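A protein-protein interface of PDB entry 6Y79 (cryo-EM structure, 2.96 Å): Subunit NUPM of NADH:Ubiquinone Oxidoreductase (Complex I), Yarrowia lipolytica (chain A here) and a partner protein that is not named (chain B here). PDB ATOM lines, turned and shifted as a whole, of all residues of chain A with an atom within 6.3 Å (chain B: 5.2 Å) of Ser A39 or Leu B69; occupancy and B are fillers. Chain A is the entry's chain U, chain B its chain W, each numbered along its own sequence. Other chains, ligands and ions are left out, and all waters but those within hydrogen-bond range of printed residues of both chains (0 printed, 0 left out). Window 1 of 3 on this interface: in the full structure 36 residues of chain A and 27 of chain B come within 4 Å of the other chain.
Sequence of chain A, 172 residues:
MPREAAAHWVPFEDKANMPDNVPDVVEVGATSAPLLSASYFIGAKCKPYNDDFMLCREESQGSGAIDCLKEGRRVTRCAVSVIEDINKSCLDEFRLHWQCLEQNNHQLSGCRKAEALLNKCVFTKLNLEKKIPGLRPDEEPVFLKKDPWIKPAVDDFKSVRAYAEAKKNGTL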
ATOM      1  N   SER A  32     -25.910  20.551  13.389  1.00  0.00           N
ATOM      2  CA  SER A  32     -25.994  19.111  13.103  1.00  0.00           C
ATOM      3  C   SER A  32     -24.656  18.402  13.161  1.00  0.00           C
ATOM      4  O   SER A  32     -24.597  17.237  13.556  1.00  0.00           O
ATOM      5  CB  SER A  32     -26.577  18.853  11.719  1.00  0.00           C
ATOM      6  OG  SER A  32     -25.769  19.374  10.681  1.00  0.00           O
ATOM      7  N   PRO A  34     -21.859  19.369  15.010  1.00  0.00           N
ATOM      8  CA  PRO A  34     -21.511  19.152  16.423  1.00  0.00           C
ATOM      9  C   PRO A  34     -22.496  18.282  17.187  1.00  0.00           C
ATOM     10  O   PRO A  34     -22.092  17.625  18.151  1.00  0.00           O
ATOM     11  CB  PRO A  34     -21.459  20.571  16.996  1.00  0.00           C
ATOM     12  CG  PRO A  34     -21.184  21.418  15.854  1.00  0.00           C
ATOM     13  CD  PRO A  34     -21.942  20.825  14.745  1.00  0.00           C
ATOM     14  N   LEU A  35     -23.770  18.262  16.798  1.00  0.00           N
ATOM     15  CA  LEU A  35     -24.751  17.416  17.470  1.00  0.00           C
ATOM     16  C   LEU A  35     -24.546  15.949  17.120  1.00  0.00           C
ATOM     17  O   LEU A  35     -24.646  15.075  17.985  1.00  0.00           O
ATOM     18  CB  LEU A  35     -26.158  17.863  17.084  1.00  0.00           C
ATOM     19  CG  LEU A  35     -27.398  17.647  17.934  1.00  0.00           C
ATOM     20  CD1 LEU A  35     -27.184  18.133  19.345  1.00  0.00           C
ATOM     21  CD2 LEU A  35     -28.549  18.384  17.283  1.00  0.00           C
ATOM     22  N   LEU A  36     -24.255  15.676  15.850  1.00  0.00           N
ATOM     23  CA  LEU A  36     -23.972  14.330  15.380  1.00  0.00           C
ATOM     24  C   LEU A  36     -22.626  13.844  15.877  1.00  0.00           C
ATOM     25  O   LEU A  36     -22.428  12.637  16.060  1.00  0.00           O
ATOM     26  CB  LEU A  36     -24.011  14.318  13.856  1.00  0.00           C
ATOM     27  CG  LEU A  36     -23.881  12.992  13.123  1.00  0.00           C
ATOM     28  CD1 LEU A  36     -24.999  12.071  13.550  1.00  0.00           C
ATOM     29  CD2 LEU A  36     -23.911  13.225  11.631  1.00  0.00           C
ATOM     30  N   SER A  37     -21.694  14.768  16.092  1.00  0.00           N
ATOM     31  CA  SER A  37     -20.393  14.417  16.636  1.00  0.00           C
ATOM     32  C   SER A  37     -20.508  13.915  18.064  1.00  0.00           C
ATOM     33  O   SER A  37     -19.973  12.856  18.409  1.00  0.00           O
ATOM     34  CB  SER A  37     -19.488  15.634  16.566  1.00  0.00           C
ATOM     35  OG  SER A  37     -19.042  15.813  15.243  1.00  0.00           O
ATOM     36  N   ALA A  38     -21.213  14.658  18.905  1.00  0.00           N
ATOM     37  CA  ALA A  38     -21.308  14.339  20.316  1.00  0.00           C
ATOM     38  C   ALA A  38     -22.566  13.573  20.661  1.00  0.00           C
ATOM     39  O   ALA A  38     -22.925  13.520  21.835  1.00  0.00           O
ATOM     40  CB  ALA A  38     -21.246  15.617  21.141  1.00  0.00           C
ATOM     41  N   SER A  39     -23.225  12.972  19.668  1.00  0.00           N
ATOM     42  CA  SER A  39     -24.477  12.257  19.885  1.00  0.00           C
ATOM     43  C   SER A  39     -24.291  11.075  20.819  1.00  0.00           C
ATOM     44  O   SER A  39     -25.132  10.832  21.688  1.00  0.00           O
ATOM     45  CB  SER A  39     -25.047  11.781  18.551  1.00  0.00           C
ATOM     46  OG  SER A  39     -26.204  10.994  18.769  1.00  0.00           O
ATOM     47  N   TYR A  40     -23.183  10.355  20.682  1.00  0.00           N
ATOM     48  CA  TYR A  40     -22.980   9.159  21.487  1.00  0.00           C
ATOM     49  C   TYR A  40     -22.620   9.501  22.916  1.00  0.00           C
ATOM     50  O   TYR A  40     -22.935   8.741  23.831  1.00  0.00           O
ATOM     51  CB  TYR A  40     -21.906   8.283  20.857  1.00  0.00           C
ATOM     52  CG  TYR A  40     -22.369   7.721  19.549  1.00  0.00           C
ATOM     53  CD1 TYR A  40     -23.069   6.526  19.502  1.00  0.00           C
ATOM     54  CD2 TYR A  40     -22.147   8.405  18.365  1.00  0.00           C
ATOM     55  CE1 TYR A  40     -23.511   6.022  18.317  1.00  0.00           C
ATOM     56  CE2 TYR A  40     -22.587   7.913  17.182  1.00  0.00           C
ATOM     57  CZ  TYR A  40     -23.268   6.725  17.167  1.00  0.00           C
ATOM     58  OH  TYR A  40     -23.705   6.234  15.980  1.00  0.00           O
ATOM     59  N   PHE A  41     -22.015  10.658  23.137  1.00  0.00           N
ATOM     60  CA  PHE A  41     -21.667  11.074  24.483  1.00  0.00           C
ATOM     61  C   PHE A  41     -22.836  11.751  25.189  1.00  0.00           C
ATOM     62  O   PHE A  41     -23.007  11.551  26.410  1.00  0.00           O
ATOM     63  CB  PHE A  41     -20.422  11.958  24.410  1.00  0.00           C
ATOM     64  CG  PHE A  41     -19.226  11.250  23.818  1.00  0.00           C
ATOM     65  CD1 PHE A  41     -18.609  10.225  24.511  1.00  0.00           C
ATOM     66  CD2 PHE A  41     -18.741  11.586  22.566  1.00  0.00           C
ATOM     67  CE1 PHE A  41     -17.519   9.555  23.974  1.00  0.00           C
ATOM     68  CE2 PHE A  41     -17.647  10.922  22.026  1.00  0.00           C
ATOM     69  CZ  PHE A  41     -17.038   9.909  22.733  1.00  0.00           C
ATOM     70  N   ILE A  42     -23.671  12.481  24.435  1.00  0.00           N
ATOM     71  CA  ILE A  42     -24.982  12.869  24.945  1.00  0.00           C
ATOM     72  C   ILE A  42     -25.786  11.631  25.341  1.00  0.00           C
ATOM     73  O   ILE A  42     -26.353  11.581  26.431  1.00  0.00           O
ATOM     74  CB  ILE A  42     -25.727  13.719  23.897  1.00  0.00           C
ATOM     75  CG1 ILE A  42     -25.064  15.092  23.689  1.00  0.00           C
ATOM     76  CG2 ILE A  42     -27.188  13.879  24.265  1.00  0.00           C
ATOM     77  CD1 ILE A  42     -25.534  15.751  22.413  1.00  0.00           C
ATOM     78  N   GLY A  43     -25.778  10.582  24.516  1.00  0.00           N
ATOM     79  CA  GLY A  43     -26.495   9.363  24.856  1.00  0.00           C
ATOM     80  C   GLY A  43     -25.880   8.553  25.978  1.00  0.00           C
ATOM     81  O   GLY A  43     -26.590   7.824  26.675  1.00  0.00           O
ATOM     82  N   ALA A  44     -24.566   8.651  26.163  1.00  0.00           N
ATOM     83  CA  ALA A  44     -23.913   7.918  27.241  1.00  0.00           C
ATOM     84  C   ALA A  44     -24.177   8.568  28.590  1.00  0.00           C
ATOM     85  O   ALA A  44     -24.433   7.869  29.579  1.00  0.00           O
ATOM     86  CB  ALA A  44     -22.414   7.823  26.978  1.00  0.00           C
ATOM     87  N   TRP B  64     -28.424   4.558  15.821  1.00  0.00           N
ATOM     88  CA  TRP B  64     -28.291   4.785  17.261  1.00  0.00           C
ATOM     89  C   TRP B  64     -27.888   6.225  17.569  1.00  0.00           C
ATOM     90  O   TRP B  64     -28.299   6.767  18.603  1.00  0.00           O
ATOM     91  CB  TRP B  64     -27.295   3.802  17.884  1.00  0.00           C
ATOM     92  CG  TRP B  64     -27.783   2.375  17.925  1.00  0.00           C
ATOM     93  CD1 TRP B  64     -27.444   1.378  17.077  1.00  0.00           C
ATOM     94  CD2 TRP B  64     -28.686   1.795  18.869  1.00  0.00           C
ATOM     95  NE1 TRP B  64     -28.083   0.218  17.411  1.00  0.00           N
ATOM     96  CE2 TRP B  64     -28.851   0.448  18.516  1.00  0.00           C
ATOM     97  CE3 TRP B  64     -29.353   2.278  19.988  1.00  0.00           C
ATOM     98  CZ2 TRP B  64     -29.672  -0.412  19.230  1.00  0.00           C
ATOM     99  CZ3 TRP B  64     -30.188   1.434  20.679  1.00  0.00           C
ATOM    100  CH2 TRP B  64     -30.328   0.100  20.310  1.00  0.00           C
ATOM    101  N   ALA B  65     -27.148   6.879  16.662  1.00  0.00           N
ATOM    102  CA  ALA B  65     -26.864   8.305  16.832  1.00  0.00           C
ATOM    103  C   ALA B  65     -28.134   9.154  16.792  1.00  0.00           C
ATOM    104  O   ALA B  65     -28.322  10.051  17.630  1.00  0.00           O
ATOM    105  CB  ALA B  65     -25.891   8.773  15.754  1.00  0.00           C
ATOM    106  N   ARG B  66     -29.027   8.871  15.840  1.00  0.00           N
ATOM    107  CA  ARG B  66     -30.250   9.663  15.720  1.00  0.00           C
ATOM    108  C   ARG B  66     -31.189   9.445  16.898  1.00  0.00           C
ATOM    109  O   ARG B  66     -31.863  10.382  17.343  1.00  0.00           O
ATOM    110  CB  ARG B  66     -30.966   9.339  14.417  1.00  0.00           C
ATOM    111  CG  ARG B  66     -30.311   9.931  13.218  1.00  0.00           C
ATOM    112  CD  ARG B  66     -31.091   9.624  11.985  1.00  0.00           C
ATOM    113  NE  ARG B  66     -30.398  10.121  10.811  1.00  0.00           N
ATOM    114  CZ  ARG B  66     -30.867  10.029   9.578  1.00  0.00           C
ATOM    115  NH1 ARG B  66     -30.161  10.512   8.569  1.00  0.00           N
ATOM    116  NH2 ARG B  66     -32.036   9.454   9.354  1.00  0.00           N
ATOM    117  N   ILE B  67     -31.247   8.226  17.434  1.00  0.00           N
ATOM    118  CA  ILE B  67     -32.127   8.072  18.588  1.00  0.00           C
ATOM    119  C   ILE B  67     -31.485   8.553  19.873  1.00  0.00           C
ATOM    120  O   ILE B  67     -32.193   8.769  20.861  1.00  0.00           O
ATOM    121  CB  ILE B  67     -32.619   6.637  18.781  1.00  0.00           C
ATOM    122  CG1 ILE B  67     -31.466   5.703  19.024  1.00  0.00           C
ATOM    123  CG2 ILE B  67     -33.391   6.208  17.602  1.00  0.00           C
ATOM    124  CD1 ILE B  67     -31.951   4.368  19.245  1.00  0.00           C
ATOM    125  N   TYR B  68     -30.165   8.715  19.910  1.00  0.00           N
ATOM    126  CA  TYR B  68     -29.592   9.474  21.014  1.00  0.00           C
ATOM    127  C   TYR B  68     -29.940  10.950  20.906  1.00  0.00           C
ATOM    128  O   TYR B  68     -30.067  11.633  21.925  1.00  0.00           O
ATOM    129  CB  TYR B  68     -28.081   9.300  21.056  1.00  0.00           C
ATOM    130  CG  TYR B  68     -27.627   7.945  21.516  1.00  0.00           C
ATOM    131  CD1 TYR B  68     -28.421   7.166  22.339  1.00  0.00           C
ATOM    132  CD2 TYR B  68     -26.401   7.442  21.119  1.00  0.00           C
ATOM    133  CE1 TYR B  68     -28.001   5.923  22.759  1.00  0.00           C
ATOM    134  CE2 TYR B  68     -25.971   6.205  21.533  1.00  0.00           C
ATOM    135  CZ  TYR B  68     -26.774   5.451  22.352  1.00  0.00           C
ATOM    136  OH  TYR B  68     -26.347   4.216  22.764  1.00  0.00           O
ATOM    137  N   LEU B  69     -30.096  11.457  19.686  1.00  0.00           N
ATOM    138  CA  LEU B  69     -30.446  12.864  19.520  1.00  0.00           C
ATOM    139  C   LEU B  69     -31.934  13.161  19.644  1.00  0.00           C
ATOM    140  O   LEU B  69     -32.286  14.333  19.791  1.00  0.00           O
ATOM    141  CB  LEU B  69     -29.982  13.372  18.162  1.00  0.00           C
ATOM    142  CG  LEU B  69     -28.480  13.372  17.949  1.00  0.00           C
ATOM    143  CD1 LEU B  69     -28.143  13.928  16.581  1.00  0.00           C
ATOM    144  CD2 LEU B  69     -27.828  14.162  19.052  1.00  0.00           C
ATOM    145  N   MET B  70     -32.804  12.150  19.537  1.00  0.00           N
ATOM    146  CA  MET B  70     -34.246  12.405  19.452  1.00  0.00           C
ATOM    147  C   MET B  70     -34.883  13.121  20.651  1.00  0.00           C
ATOM    148  O   MET B  70     -35.598  14.112  20.410  1.00  0.00           O
ATOM    149  CB  MET B  70     -34.997  11.104  19.146  1.00  0.00           C
ATOM    150  CG  MET B  70     -36.502  11.290  19.193  1.00  0.00           C
ATOM    151  SD  MET B  70     -37.484   9.822  18.952  1.00  0.00           S
ATOM    152  CE  MET B  70     -36.805   9.264  17.413  1.00  0.00           C
ATOM    153  N   PRO B  71     -34.706  12.707  21.927  1.00  0.00           N
ATOM    154  CA  PRO B  71     -35.433  13.411  23.006  1.00  0.00           C
ATOM    155  C   PRO B  71     -34.981  14.841  23.207  1.00  0.00           C
ATOM    156  O   PRO B  71     -35.782  15.683  23.631  1.00  0.00           O
ATOM    157  CB  PRO B  71     -35.135  12.564  24.251  1.00  0.00           C
ATOM    158  CG  PRO B  71     -34.654  11.288  23.746  1.00  0.00           C
ATOM    159  CD  PRO B  71     -33.907  11.614  22.516  1.00  0.00           C
ATOM    160  N   LEU B  72     -33.731  15.129  22.851  1.00  0.00           N
ATOM    161  CA  LEU B  72     -33.181  16.473  22.942  1.00  0.00           C
ATOM    162  C   LEU B  72     -33.908  17.450  22.027  1.00  0.00           C
ATOM    163  O   LEU B  72     -34.153  18.599  22.407  1.00  0.00           O
ATOM    164  CB  LEU B  72     -31.700  16.414  22.591  1.00  0.00           C
ATOM    165  CG  LEU B  72     -30.944  17.722  22.618  1.00  0.00           C
ATOM    166  CD1 LEU B  72     -31.117  18.302  23.997  1.00  0.00           C
ATOM    167  CD2 LEU B  72     -29.494  17.458  22.304  1.00  0.00           C
ATOM    168  N   LEU B  73     -34.252  17.018  20.817  1.00  0.00           N
ATOM    169  CA  LEU B  73     -34.995  17.878  19.903  1.00  0.00           C
ATOM    170  C   LEU B  73     -36.495  17.792  20.143  1.00  0.00           C
ATOM    171  O   LEU B  73     -37.239  18.725  19.809  1.00  0.00           O
ATOM    172  CB  LEU B  73     -34.671  17.495  18.465  1.00  0.00           C
ATOM    173  CG  LEU B  73     -33.183  17.489  18.142  1.00  0.00           C
ATOM    174  CD1 LEU B  73     -32.947  16.833  16.822  1.00  0.00           C
ATOM    175  CD2 LEU B  73     -32.670  18.898  18.122  1.00  0.00           C
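The side-chain hydroxyl of Ser A39 is in hydrogen-bond range of the backbone carbonyl oxygen of Ala B65 (2.6 Å).
Leu A35 touches Leu B69 (O to CD2, 3.5 Å). Leu A35 touches Leu B72 (CD1 to CD2, 3.8 Å). O of Ser A39 touches CB of Tyr B68 (3.4 Å). OG of Ser A39 touches CG of Leu B69, at 3.4 Å. CB of Ala B65 touches OH of Tyr A40, 3.4 Å away. Tyr B68 touches Tyr A40. Tyr B68 touches Gly A43.
Leu B69 touches two residues of chain A. Printed residues of chain A within 4 Å of Ala B65: Ser A39 (2.6 Å) and Tyr A40 (3.4 Å). Printed residues of chain B within 4 Å of Leu A35: Leu B69 and Leu B72. Of the printed residues of chain B, Gly A43 touches Tyr B68. The nearest printed residue of chain B that does not touch Tyr A40 is Trp B64 (4.4 Å).
Of the 10 printed residues of chain B, 4 touch a printed residue of chain A. Of the 12 printed residues of chain A, 4 touch a printed residue of chain B. Printed residues of chain A that touch a printed residue of chain B: Leu A35, Ser A39, Tyr A40 and Gly A43. Hydrophobic or aromatic side chains of chain A within 4 Å of the printed part of chain B: Leu A35 and Tyr A40. Among the printed residues, no Asp or Glu carboxylate lies within 4 Å of a Lys or Arg side-chain nitrogen of the other chain.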
